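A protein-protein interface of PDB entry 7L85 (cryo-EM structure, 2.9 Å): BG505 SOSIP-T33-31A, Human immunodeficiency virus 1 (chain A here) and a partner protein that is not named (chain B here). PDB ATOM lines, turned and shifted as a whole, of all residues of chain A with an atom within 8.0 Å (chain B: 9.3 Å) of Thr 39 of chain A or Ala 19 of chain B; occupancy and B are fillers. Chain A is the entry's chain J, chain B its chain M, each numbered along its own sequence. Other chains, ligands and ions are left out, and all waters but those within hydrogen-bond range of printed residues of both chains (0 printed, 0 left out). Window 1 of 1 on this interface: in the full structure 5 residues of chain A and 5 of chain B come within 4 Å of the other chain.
O of Val 49 of chain A lies within hydrogen-bond range of N of Tyr 42 of chain A, at 3.0 Å. The backbone carbonyl oxygen of Leu 38 of chain A lies close to a ring nitrogen (ND1) of His 52 of chain A. O of Glu 13 of chain B is in hydrogen-bond range of NE of Arg 87 of chain B. OE2 of Glu 14 of chain B sits at hydrogen-bond distance from OG1 of Thr 16 of chain B (2.7 Å).
Hydrophobic or aromatic side chains of chain B within 4 Å of the printed part of chain A: Ala 18. Hydrophobic or aromatic side chains of chain A that line the printed part of chain B: Val 49 and His 52. Among the printed residues, no Asp or Glu carboxylate lies within 4 Å of a Lys or Arg side-chain nitrogen of the other chain.
The side-chain carboxylate (OE1) of Glu 26 of chain B is in hydrogen-bond range of the backbone NH (N) of Ser 50 of chain A, at 2.9 Å.
No residue of chain B comes within 4 Å of Leu 38 of chain A. Thr 39 of chain A touches just these residues of chain B: Ala 18 (3.8 Å) and Ala 19 (3.9 Å). Ser 40 of chain A touches none of the printed residues of chain B. Printed residues of chain B within 4 Å of Ser 50 of chain A: Glu 26 (2.9 Å). Of the printed residues of chain B, His 52 of chain A touches Glu 13 (3.4 Å) and Glu 14 (3.5 Å). Of the printed residues of chain A, Glu 13 of chain B touches His 52. Of the printed residues of chain A, Glu 14 of chain B touches His 52 (3.5 Å). Thr 16 of chain B touches none of the printed residues of chain A. Of chain A, only Thr 39 (3.9 Å) comes within 4 Å of Ala 19 of chain B. Ile 20 of chain B touches none of the printed residues of chain A. The nearest printed residue of chain B that does not touch Ser 50 of chain A is Ala 22 of chain B (4.1 Å).
Among the printed residues, merely in contact across the chains: His 52 of chain A with Glu 13 of chain B, Val 49 of chain A with Glu 26 of chain B, His 52 of chain A with Glu 14 of chain B, Thr 39 of chain A with Ala 18 of chain B and Thr 39 of chain A with Ala 19 of chain B.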
ATOM      1  N   PRO A  36     -32.910 -14.823 -17.319  1.00  0.00           N
ATOM      2  CA  PRO A  36     -32.040 -13.780 -17.800  1.00  0.00           C
ATOM      3  C   PRO A  36     -31.570 -14.011 -19.204  1.00  0.00           C
ATOM      4  O   PRO A  36     -31.660 -15.129 -19.696  1.00  0.00           O
ATOM      5  CB  PRO A  36     -30.880 -13.879 -16.842  1.00  0.00           C
ATOM      6  CG  PRO A  36     -30.806 -15.333 -16.548  1.00  0.00           C
ATOM      7  CD  PRO A  36     -32.224 -15.809 -16.517  1.00  0.00           C
ATOM      8  N   GLY A  37     -30.979 -12.982 -19.800  1.00  0.00           N
ATOM      9  CA  GLY A  37     -30.240 -13.151 -21.040  1.00  0.00           C
ATOM     10  C   GLY A  37     -31.021 -13.275 -22.325  1.00  0.00           C
ATOM     11  O   GLY A  37     -30.543 -13.927 -23.246  1.00  0.00           O
ATOM     12  N   LEU A  38     -32.192 -12.697 -22.412  1.00  0.00           N
ATOM     13  CA  LEU A  38     -32.950 -12.835 -23.628  1.00  0.00           C
ATOM     14  C   LEU A  38     -32.507 -11.860 -24.669  1.00  0.00           C
ATOM     15  O   LEU A  38     -31.857 -10.866 -24.377  1.00  0.00           O
ATOM     16  CB  LEU A  38     -34.435 -12.644 -23.375  1.00  0.00           C
ATOM     17  CG  LEU A  38     -35.225 -13.858 -23.006  1.00  0.00           C
ATOM     18  CD1 LEU A  38     -34.719 -14.496 -21.737  1.00  0.00           C
ATOM     19  CD2 LEU A  38     -36.629 -13.445 -22.828  1.00  0.00           C
ATOM     20  N   THR A  39     -32.772 -12.199 -25.912  1.00  0.00           N
ATOM     21  CA  THR A  39     -32.584 -11.260 -26.997  1.00  0.00           C
ATOM     22  C   THR A  39     -33.957 -11.044 -27.575  1.00  0.00           C
ATOM     23  O   THR A  39     -34.681 -11.987 -27.874  1.00  0.00           O
ATOM     24  CB  THR A  39     -31.576 -11.757 -28.041  1.00  0.00           C
ATOM     25  OG1 THR A  39     -30.315 -11.945 -27.403  1.00  0.00           O
ATOM     26  CG2 THR A  39     -31.427 -10.765 -29.177  1.00  0.00           C
ATOM     27  N   SER A  40     -34.354  -9.811 -27.696  1.00  0.00           N
ATOM     28  CA  SER A  40     -35.703  -9.518 -28.149  1.00  0.00           C
ATOM     29  C   SER A  40     -35.796  -8.790 -29.445  1.00  0.00           C
ATOM     30  O   SER A  40     -35.240  -7.715 -29.591  1.00  0.00           O
ATOM     31  CB  SER A  40     -36.358  -8.705 -27.096  1.00  0.00           C
ATOM     32  OG  SER A  40     -37.612  -8.231 -27.489  1.00  0.00           O
ATOM     33  N   ILE A  41     -36.465  -9.390 -30.415  1.00  0.00           N
ATOM     34  CA  ILE A  41     -36.652  -8.770 -31.717  1.00  0.00           C
ATOM     35  C   ILE A  41     -38.104  -8.436 -31.877  1.00  0.00           C
ATOM     36  O   ILE A  41     -38.956  -9.312 -31.814  1.00  0.00           O
ATOM     37  CB  ILE A  41     -36.184  -9.683 -32.845  1.00  0.00           C
ATOM     38  CG1 ILE A  41     -34.687  -9.953 -32.666  1.00  0.00           C
ATOM     39  CG2 ILE A  41     -36.499  -9.051 -34.183  1.00  0.00           C
ATOM     40  CD1 ILE A  41     -34.115 -11.021 -33.553  1.00  0.00           C
ATOM     41  N   TYR A  42     -38.418  -7.186 -32.088  1.00  0.00           N
ATOM     42  CA  TYR A  42     -39.822  -6.854 -32.153  1.00  0.00           C
ATOM     43  C   TYR A  42     -40.111  -5.686 -33.020  1.00  0.00           C
ATOM     44  O   TYR A  42     -39.229  -4.897 -33.356  1.00  0.00           O
ATOM     45  CB  TYR A  42     -40.344  -6.618 -30.759  1.00  0.00           C
ATOM     46  CG  TYR A  42     -39.762  -5.472 -30.112  1.00  0.00           C
ATOM     47  CD1 TYR A  42     -40.398  -4.298 -30.142  1.00  0.00           C
ATOM     48  CD2 TYR A  42     -38.572  -5.586 -29.482  1.00  0.00           C
ATOM     49  CE1 TYR A  42     -39.856  -3.226 -29.549  1.00  0.00           C
ATOM     50  CE2 TYR A  42     -38.025  -4.517 -28.891  1.00  0.00           C
ATOM     51  CZ  TYR A  42     -38.664  -3.327 -28.928  1.00  0.00           C
ATOM     52  OH  TYR A  42     -38.108  -2.219 -28.328  1.00  0.00           O
ATOM     53  N   VAL A  49     -36.633  -3.797 -34.470  1.00  0.00           N
ATOM     54  CA  VAL A  49     -35.528  -3.426 -33.623  1.00  0.00           C
ATOM     55  C   VAL A  49     -35.220  -4.490 -32.627  1.00  0.00           C
ATOM     56  O   VAL A  49     -36.064  -5.347 -32.363  1.00  0.00           O
ATOM     57  CB  VAL A  49     -35.880  -2.162 -32.856  1.00  0.00           C
ATOM     58  CG1 VAL A  49     -36.184  -1.062 -33.814  1.00  0.00           C
ATOM     59  CG2 VAL A  49     -37.062  -2.417 -31.956  1.00  0.00           C
ATOM     60  N   SER A  50     -34.039  -4.437 -32.029  1.00  0.00           N
ATOM     61  CA  SER A  50     -33.768  -5.385 -30.972  1.00  0.00           C
ATOM     62  C   SER A  50     -33.532  -4.734 -29.621  1.00  0.00           C
ATOM     63  O   SER A  50     -33.203  -3.555 -29.512  1.00  0.00           O
ATOM     64  CB  SER A  50     -32.588  -6.254 -31.288  1.00  0.00           C
ATOM     65  OG  SER A  50     -31.410  -5.518 -31.298  1.00  0.00           O
ATOM     66  N   ASP A  51     -33.685  -5.533 -28.581  1.00  0.00           N
ATOM     67  CA  ASP A  51     -33.441  -5.141 -27.200  1.00  0.00           C
ATOM     68  C   ASP A  51     -32.881  -6.316 -26.423  1.00  0.00           C
ATOM     69  O   ASP A  51     -32.646  -7.380 -26.993  1.00  0.00           O
ATOM     70  CB  ASP A  51     -34.744  -4.629 -26.575  1.00  0.00           C
ATOM     71  CG  ASP A  51     -34.573  -3.702 -25.370  1.00  0.00           C
ATOM     72  OD1 ASP A  51     -33.500  -3.683 -24.814  1.00  0.00           O
ATOM     73  OD2 ASP A  51     -35.522  -3.090 -24.958  1.00  0.00           O
ATOM     74  N   HIS A  52     -32.599  -6.126 -25.147  1.00  0.00           N
ATOM     75  CA  HIS A  52     -32.080  -7.214 -24.331  1.00  0.00           C
ATOM     76  C   HIS A  52     -33.194  -8.003 -23.665  1.00  0.00           C
ATOM     77  O   HIS A  52     -33.697  -8.953 -24.244  1.00  0.00           O
ATOM     78  CB  HIS A  52     -31.109  -6.663 -23.291  1.00  0.00           C
ATOM     79  CG  HIS A  52     -30.577  -7.676 -22.366  1.00  0.00           C
ATOM     80  ND1 HIS A  52     -29.726  -8.656 -22.760  1.00  0.00           N
ATOM     81  CD2 HIS A  52     -30.775  -7.854 -21.043  1.00  0.00           C
ATOM     82  CE1 HIS A  52     -29.423  -9.399 -21.721  1.00  0.00           C
ATOM     83  NE2 HIS A  52     -30.055  -8.935 -20.671  1.00  0.00           N
ATOM     84  N   GLU A  53     -33.675  -7.518 -22.535  1.00  0.00           N
ATOM     85  CA  GLU A  53     -34.763  -8.111 -21.755  1.00  0.00           C
ATOM     86  C   GLU A  53     -34.461  -9.398 -20.955  1.00  0.00           C
ATOM     87  O   GLU A  53     -33.547 -10.180 -21.232  1.00  0.00           O
ATOM     88  CB  GLU A  53     -35.963  -8.414 -22.654  1.00  0.00           C
ATOM     89  CG  GLU A  53     -36.584  -7.204 -23.346  1.00  0.00           C
ATOM     90  CD  GLU A  53     -37.638  -7.638 -24.304  1.00  0.00           C
ATOM     91  OE1 GLU A  53     -37.838  -8.823 -24.366  1.00  0.00           O
ATOM     92  OE2 GLU A  53     -38.205  -6.852 -25.026  1.00  0.00           O
ATOM     93  N   LEU A  54     -35.277  -9.575 -19.926  1.00  0.00           N
ATOM     94  CA  LEU A  54     -35.367 -10.748 -19.069  1.00  0.00           C
ATOM     95  C   LEU A  54     -36.811 -11.187 -19.033  1.00  0.00           C
ATOM     96  O   LEU A  54     -37.715 -10.380 -19.232  1.00  0.00           O
ATOM     97  CB  LEU A  54     -34.963 -10.472 -17.632  1.00  0.00           C
ATOM     98  CG  LEU A  54     -33.585 -10.036 -17.360  1.00  0.00           C
ATOM     99  CD1 LEU A  54     -33.515  -8.562 -17.401  1.00  0.00           C
ATOM    100  CD2 LEU A  54     -33.193 -10.510 -15.996  1.00  0.00           C
ATOM    101  N   ILE B  10     -23.988   0.797 -33.831  1.00  0.00           N
ATOM    102  CA  ILE B  10     -24.974   0.331 -32.879  1.00  0.00           C
ATOM    103  C   ILE B  10     -24.306  -0.287 -31.690  1.00  0.00           C
ATOM    104  O   ILE B  10     -23.228  -0.863 -31.817  1.00  0.00           O
ATOM    105  CB  ILE B  10     -25.914  -0.670 -33.554  1.00  0.00           C
ATOM    106  CG1 ILE B  10     -27.082  -1.000 -32.658  1.00  0.00           C
ATOM    107  CG2 ILE B  10     -25.154  -1.929 -33.906  1.00  0.00           C
ATOM    108  CD1 ILE B  10     -28.235  -1.664 -33.355  1.00  0.00           C
ATOM    109  N   THR B  11     -24.923  -0.191 -30.536  1.00  0.00           N
ATOM    110  CA  THR B  11     -24.359  -0.850 -29.380  1.00  0.00           C
ATOM    111  C   THR B  11     -25.199  -2.012 -28.941  1.00  0.00           C
ATOM    112  O   THR B  11     -26.414  -2.036 -29.142  1.00  0.00           O
ATOM    113  CB  THR B  11     -24.258   0.112 -28.212  1.00  0.00           C
ATOM    114  OG1 THR B  11     -25.572   0.536 -27.806  1.00  0.00           O
ATOM    115  CG2 THR B  11     -23.514   1.266 -28.647  1.00  0.00           C
ATOM    116  N   VAL B  12     -24.575  -2.925 -28.220  1.00  0.00           N
ATOM    117  CA  VAL B  12     -25.299  -4.051 -27.654  1.00  0.00           C
ATOM    118  C   VAL B  12     -25.042  -4.100 -26.179  1.00  0.00           C
ATOM    119  O   VAL B  12     -24.075  -3.509 -25.718  1.00  0.00           O
ATOM    120  CB  VAL B  12     -24.886  -5.376 -28.306  1.00  0.00           C
ATOM    121  CG1 VAL B  12     -25.169  -5.329 -29.744  1.00  0.00           C
ATOM    122  CG2 VAL B  12     -23.451  -5.656 -28.089  1.00  0.00           C
ATOM    123  N   GLU B  13     -25.882  -4.798 -25.427  1.00  0.00           N
ATOM    124  CA  GLU B  13     -25.657  -4.873 -23.994  1.00  0.00           C
ATOM    125  C   GLU B  13     -24.770  -6.015 -23.554  1.00  0.00           C
ATOM    126  O   GLU B  13     -24.209  -5.974 -22.461  1.00  0.00           O
ATOM    127  CB  GLU B  13     -26.966  -4.900 -23.244  1.00  0.00           C
ATOM    128  CG  GLU B  13     -27.740  -3.623 -23.422  1.00  0.00           C
ATOM    129  CD  GLU B  13     -28.953  -3.539 -22.581  1.00  0.00           C
ATOM    130  OE1 GLU B  13     -29.120  -4.378 -21.737  1.00  0.00           O
ATOM    131  OE2 GLU B  13     -29.718  -2.632 -22.774  1.00  0.00           O
ATOM    132  N   GLU B  14     -24.667  -7.057 -24.354  1.00  0.00           N
ATOM    133  CA  GLU B  14     -23.833  -8.170 -23.959  1.00  0.00           C
ATOM    134  C   GLU B  14     -23.234  -8.891 -25.141  1.00  0.00           C
ATOM    135  O   GLU B  14     -23.769  -8.868 -26.248  1.00  0.00           O
ATOM    136  CB  GLU B  14     -24.598  -9.145 -23.101  1.00  0.00           C
ATOM    137  CG  GLU B  14     -25.729  -9.796 -23.771  1.00  0.00           C
ATOM    138  CD  GLU B  14     -26.389 -10.760 -22.877  1.00  0.00           C
ATOM    139  OE1 GLU B  14     -26.199 -10.673 -21.693  1.00  0.00           O
ATOM    140  OE2 GLU B  14     -27.073 -11.622 -23.369  1.00  0.00           O
ATOM    141  N   ASP B  15     -22.144  -9.603 -24.906  1.00  0.00           N
ATOM    142  CA  ASP B  15     -21.492 -10.351 -25.963  1.00  0.00           C
ATOM    143  C   ASP B  15     -22.114 -11.723 -26.152  1.00  0.00           C
ATOM    144  O   ASP B  15     -21.518 -12.747 -25.823  1.00  0.00           O
ATOM    145  CB  ASP B  15     -20.013 -10.496 -25.634  1.00  0.00           C
ATOM    146  CG  ASP B  15     -19.147 -11.012 -26.768  1.00  0.00           C
ATOM    147  OD1 ASP B  15     -19.586 -11.109 -27.901  1.00  0.00           O
ATOM    148  OD2 ASP B  15     -17.991 -11.255 -26.528  1.00  0.00           O
ATOM    149  N   THR B  16     -23.308 -11.714 -26.685  1.00  0.00           N
ATOM    150  CA  THR B  16     -24.087 -12.901 -26.977  1.00  0.00           C
ATOM    151  C   THR B  16     -24.280 -12.952 -28.470  1.00  0.00           C
ATOM    152  O   THR B  16     -24.800 -11.985 -29.023  1.00  0.00           O
ATOM    153  CB  THR B  16     -25.435 -12.870 -26.253  1.00  0.00           C
ATOM    154  OG1 THR B  16     -25.204 -12.871 -24.861  1.00  0.00           O
ATOM    155  CG2 THR B  16     -26.296 -14.039 -26.618  1.00  0.00           C
ATOM    156  N   PRO B  17     -23.960 -14.046 -29.169  1.00  0.00           N
ATOM    157  CA  PRO B  17     -24.079 -14.146 -30.596  1.00  0.00           C
ATOM    158  C   PRO B  17     -25.404 -13.693 -31.124  1.00  0.00           C
ATOM    159  O   PRO B  17     -25.461 -13.011 -32.139  1.00  0.00           O
ATOM    160  CB  PRO B  17     -23.929 -15.634 -30.811  1.00  0.00           C
ATOM    161  CG  PRO B  17     -23.050 -16.065 -29.726  1.00  0.00           C
ATOM    162  CD  PRO B  17     -23.469 -15.255 -28.537  1.00  0.00           C
ATOM    163  N   ALA B  18     -26.481 -13.997 -30.421  1.00  0.00           N
ATOM    164  CA  ALA B  18     -27.761 -13.567 -30.914  1.00  0.00           C
ATOM    165  C   ALA B  18     -27.881 -12.066 -30.900  1.00  0.00           C
ATOM    166  O   ALA B  18     -28.516 -11.493 -31.782  1.00  0.00           O
ATOM    167  CB  ALA B  18     -28.871 -14.168 -30.096  1.00  0.00           C
ATOM    168  N   ALA B  19     -27.303 -11.414 -29.897  1.00  0.00           N
ATOM    169  CA  ALA B  19     -27.426  -9.982 -29.779  1.00  0.00           C
ATOM    170  C   ALA B  19     -26.608  -9.307 -30.828  1.00  0.00           C
ATOM    171  O   ALA B  19     -27.009  -8.291 -31.389  1.00  0.00           O
ATOM    172  CB  ALA B  19     -26.990  -9.535 -28.413  1.00  0.00           C
ATOM    173  N   ILE B  20     -25.465  -9.886 -31.122  1.00  0.00           N
ATOM    174  CA  ILE B  20     -24.601  -9.304 -32.110  1.00  0.00           C
ATOM    175  C   ILE B  20     -25.226  -9.399 -33.454  1.00  0.00           C
ATOM    176  O   ILE B  20     -25.184  -8.438 -34.228  1.00  0.00           O
ATOM    177  CB  ILE B  20     -23.245  -9.974 -32.112  1.00  0.00           C
ATOM    178  CG1 ILE B  20     -22.577  -9.634 -30.823  1.00  0.00           C
ATOM    179  CG2 ILE B  20     -22.417  -9.548 -33.349  1.00  0.00           C
ATOM    180  CD1 ILE B  20     -21.385 -10.426 -30.539  1.00  0.00           C
ATOM    181  N   LEU B  21     -25.758 -10.561 -33.776  1.00  0.00           N
ATOM    182  CA  LEU B  21     -26.354 -10.723 -35.064  1.00  0.00           C
ATOM    183  C   LEU B  21     -27.586  -9.881 -35.185  1.00  0.00           C
ATOM    184  O   LEU B  21     -27.797  -9.243 -36.214  1.00  0.00           O
ATOM    185  CB  LEU B  21     -26.737 -12.165 -35.245  1.00  0.00           C
ATOM    186  CG  LEU B  21     -25.628 -13.173 -35.359  1.00  0.00           C
ATOM    187  CD1 LEU B  21     -26.261 -14.528 -35.260  1.00  0.00           C
ATOM    188  CD2 LEU B  21     -24.876 -13.019 -36.665  1.00  0.00           C
ATOM    189  N   ALA B  22     -28.406  -9.827 -34.147  1.00  0.00           N
ATOM    190  CA  ALA B  22     -29.606  -9.052 -34.262  1.00  0.00           C
ATOM    191  C   ALA B  22     -29.301  -7.587 -34.417  1.00  0.00           C
ATOM    192  O   ALA B  22     -29.923  -6.904 -35.229  1.00  0.00           O
ATOM    193  CB  ALA B  22     -30.461  -9.265 -33.049  1.00  0.00           C
ATOM    194  N   ALA B  23     -28.318  -7.094 -33.673  1.00  0.00           N
ATOM    195  CA  ALA B  23     -27.954  -5.707 -33.754  1.00  0.00           C
ATOM    196  C   ALA B  23     -27.367  -5.377 -35.086  1.00  0.00           C
ATOM    197  O   ALA B  23     -27.633  -4.315 -35.643  1.00  0.00           O
ATOM    198  CB  ALA B  23     -26.975  -5.389 -32.673  1.00  0.00           C
ATOM    199  N   THR B  24     -26.591  -6.288 -35.632  1.00  0.00           N
ATOM    200  CA  THR B  24     -25.985  -6.026 -36.899  1.00  0.00           C
ATOM    201  C   THR B  24     -27.052  -5.919 -37.945  1.00  0.00           C
ATOM    202  O   THR B  24     -26.990  -5.029 -38.789  1.00  0.00           O
ATOM    203  CB  THR B  24     -24.968  -7.077 -37.257  1.00  0.00           C
ATOM    204  OG1 THR B  24     -23.959  -7.095 -36.264  1.00  0.00           O
ATOM    205  CG2 THR B  24     -24.339  -6.702 -38.567  1.00  0.00           C
ATOM    206  N   ILE B  25     -28.055  -6.786 -37.897  1.00  0.00           N
ATOM    207  CA  ILE B  25     -29.102  -6.684 -38.883  1.00  0.00           C
ATOM    208  C   ILE B  25     -29.816  -5.381 -38.751  1.00  0.00           C
ATOM    209  O   ILE B  25     -30.059  -4.714 -39.752  1.00  0.00           O
ATOM    210  CB  ILE B  25     -30.137  -7.792 -38.765  1.00  0.00           C
ATOM    211  CG1 ILE B  25     -29.514  -9.065 -39.142  1.00  0.00           C
ATOM    212  CG2 ILE B  25     -31.337  -7.468 -39.598  1.00  0.00           C
ATOM    213  CD1 ILE B  25     -30.319 -10.265 -38.832  1.00  0.00           C
ATOM    214  N   GLU B  26     -30.168  -4.987 -37.538  1.00  0.00           N
ATOM    215  CA  GLU B  26     -30.879  -3.744 -37.401  1.00  0.00           C
ATOM    216  C   GLU B  26     -30.101  -2.604 -37.988  1.00  0.00           C
ATOM    217  O   GLU B  26     -30.657  -1.789 -38.723  1.00  0.00           O
ATOM    218  CB  GLU B  26     -31.171  -3.452 -35.941  1.00  0.00           C
ATOM    219  CG  GLU B  26     -31.915  -2.161 -35.702  1.00  0.00           C
ATOM    220  CD  GLU B  26     -32.277  -1.950 -34.269  1.00  0.00           C
ATOM    221  OE1 GLU B  26     -32.131  -2.868 -33.498  1.00  0.00           O
ATOM    222  OE2 GLU B  26     -32.720  -0.887 -33.937  1.00  0.00           O
ATOM    223  N   LEU B  27     -28.809  -2.547 -37.721  1.00  0.00           N
ATOM    224  CA  LEU B  27     -28.043  -1.452 -38.243  1.00  0.00           C
ATOM    225  C   LEU B  27     -27.915  -1.496 -39.741  1.00  0.00           C
ATOM    226  O   LEU B  27     -28.042  -0.462 -40.392  1.00  0.00           O
ATOM    227  CB  LEU B  27     -26.649  -1.441 -37.650  1.00  0.00           C
ATOM    228  CG  LEU B  27     -25.730  -0.319 -38.107  1.00  0.00           C
ATOM    229  CD1 LEU B  27     -26.309   1.037 -37.730  1.00  0.00           C
ATOM    230  CD2 LEU B  27     -24.385  -0.510 -37.495  1.00  0.00           C
ATOM    231  N   LEU B  54     -16.371  -7.523 -27.888  1.00  0.00           N
ATOM    232  CA  LEU B  54     -17.349  -8.350 -28.574  1.00  0.00           C
ATOM    233  C   LEU B  54     -16.663  -9.406 -29.388  1.00  0.00           C
ATOM    234  O   LEU B  54     -16.226  -9.138 -30.506  1.00  0.00           O
ATOM    235  CB  LEU B  54     -18.240  -7.541 -29.511  1.00  0.00           C
ATOM    236  CG  LEU B  54     -19.054  -6.442 -28.911  1.00  0.00           C
ATOM    237  CD1 LEU B  54     -19.754  -5.694 -30.015  1.00  0.00           C
ATOM    238  CD2 LEU B  54     -20.062  -7.005 -27.950  1.00  0.00           C
ATOM    239  N   SER B  56     -17.964 -12.933 -29.431  1.00  0.00           N
ATOM    240  CA  SER B  56     -18.712 -14.173 -29.613  1.00  0.00           C
ATOM    241  C   SER B  56     -19.241 -14.448 -31.020  1.00  0.00           C
ATOM    242  O   SER B  56     -19.689 -15.558 -31.301  1.00  0.00           O
ATOM    243  CB  SER B  56     -19.853 -14.237 -28.642  1.00  0.00           C
ATOM    244  OG  SER B  56     -20.829 -13.309 -28.955  1.00  0.00           O
ATOM    245  N   ALA B  57     -19.218 -13.467 -31.902  1.00  0.00           N
ATOM    246  CA  ALA B  57     -19.751 -13.653 -33.246  1.00  0.00           C
ATOM    247  C   ALA B  57     -19.176 -12.659 -34.216  1.00  0.00           C
ATOM    248  O   ALA B  57     -18.667 -11.615 -33.823  1.00  0.00           O
ATOM    249  CB  ALA B  57     -21.250 -13.534 -33.237  1.00  0.00           C
ATOM    250  N   PRO B  59     -20.109  -9.961 -37.025  1.00  0.00           N
ATOM    251  CA  PRO B  59     -21.182  -9.180 -37.603  1.00  0.00           C
ATOM    252  C   PRO B  59     -21.392  -9.480 -39.084  1.00  0.00           C
ATOM    253  O   PRO B  59     -22.518  -9.533 -39.579  1.00  0.00           O
ATOM    254  CB  PRO B  59     -20.669  -7.775 -37.405  1.00  0.00           C
ATOM    255  CG  PRO B  59     -19.831  -7.858 -36.199  1.00  0.00           C
ATOM    256  CD  PRO B  59     -19.151  -9.185 -36.278  1.00  0.00           C
ATOM    257  N   ALA B  62     -24.209 -11.753 -40.102  1.00  0.00           N
ATOM    258  CA  ALA B  62     -25.556 -11.216 -40.145  1.00  0.00           C
ATOM    259  C   ALA B  62     -25.867 -10.702 -41.522  1.00  0.00           C
ATOM    260  O   ALA B  62     -26.974 -10.838 -42.046  1.00  0.00           O
ATOM    261  CB  ALA B  62     -25.696 -10.101 -39.171  1.00  0.00           C
ATOM    262  N   ARG B  87     -18.815  -2.156 -26.262  1.00  0.00           N
ATOM    263  CA  ARG B  87     -19.712  -2.996 -27.031  1.00  0.00           C
ATOM    264  C   ARG B  87     -20.304  -2.334 -28.254  1.00  0.00           C
ATOM    265  O   ARG B  87     -21.517  -2.350 -28.468  1.00  0.00           O
ATOM    266  CB  ARG B  87     -20.795  -3.521 -26.149  1.00  0.00           C
ATOM    267  CG  ARG B  87     -20.290  -4.358 -25.016  1.00  0.00           C
ATOM    268  CD  ARG B  87     -21.380  -4.904 -24.261  1.00  0.00           C
ATOM    269  NE  ARG B  87     -22.179  -3.860 -23.737  1.00  0.00           N
ATOM    270  CZ  ARG B  87     -21.937  -3.178 -22.619  1.00  0.00           C
ATOM    271  NH1 ARG B  87     -20.902  -3.463 -21.865  1.00  0.00           N
ATOM    272  NH2 ARG B  87     -22.746  -2.203 -22.270  1.00  0.00           N
ATOM    273  N   ILE B  89     -20.551  -1.838 -32.414  1.00  0.00           N
ATOM    274  CA  ILE B  89     -20.380  -2.397 -33.738  1.00  0.00           C
ATOM    275  C   ILE B  89     -20.461  -1.239 -34.712  1.00  0.00           C
ATOM    276  O   ILE B  89     -21.447  -0.506 -34.721  1.00  0.00           O
ATOM    277  CB  ILE B  89     -21.486  -3.399 -34.071  1.00  0.00           C
ATOM    278  CG1 ILE B  89     -21.478  -4.532 -33.051  1.00  0.00           C
ATOM    279  CG2 ILE B  89     -21.288  -3.924 -35.503  1.00  0.00           C
ATOM    280  CD1 ILE B  89     -22.692  -5.436 -33.092  1.00  0.00           C
ATOM    281  N   ASN B 110     -29.024   3.182 -30.569  1.00  0.00           N
ATOM    282  CA  ASN B 110     -28.848   2.872 -29.168  1.00  0.00           C
ATOM    283  C   ASN B 110     -27.897   3.837 -28.503  1.00  0.00           C
ATOM    284  O   ASN B 110     -28.088   5.044 -28.603  1.00  0.00           O
ATOM    285  CB  ASN B 110     -28.413   1.445 -28.996  1.00  0.00           C
ATOM    286  CG  ASN B 110     -29.415   0.534 -29.521  1.00  0.00           C
ATOM    287  OD1 ASN B 110     -30.576   0.923 -29.672  1.00  0.00           O
ATOM    288  ND2 ASN B 110     -29.043  -0.680 -29.792  1.00  0.00           N
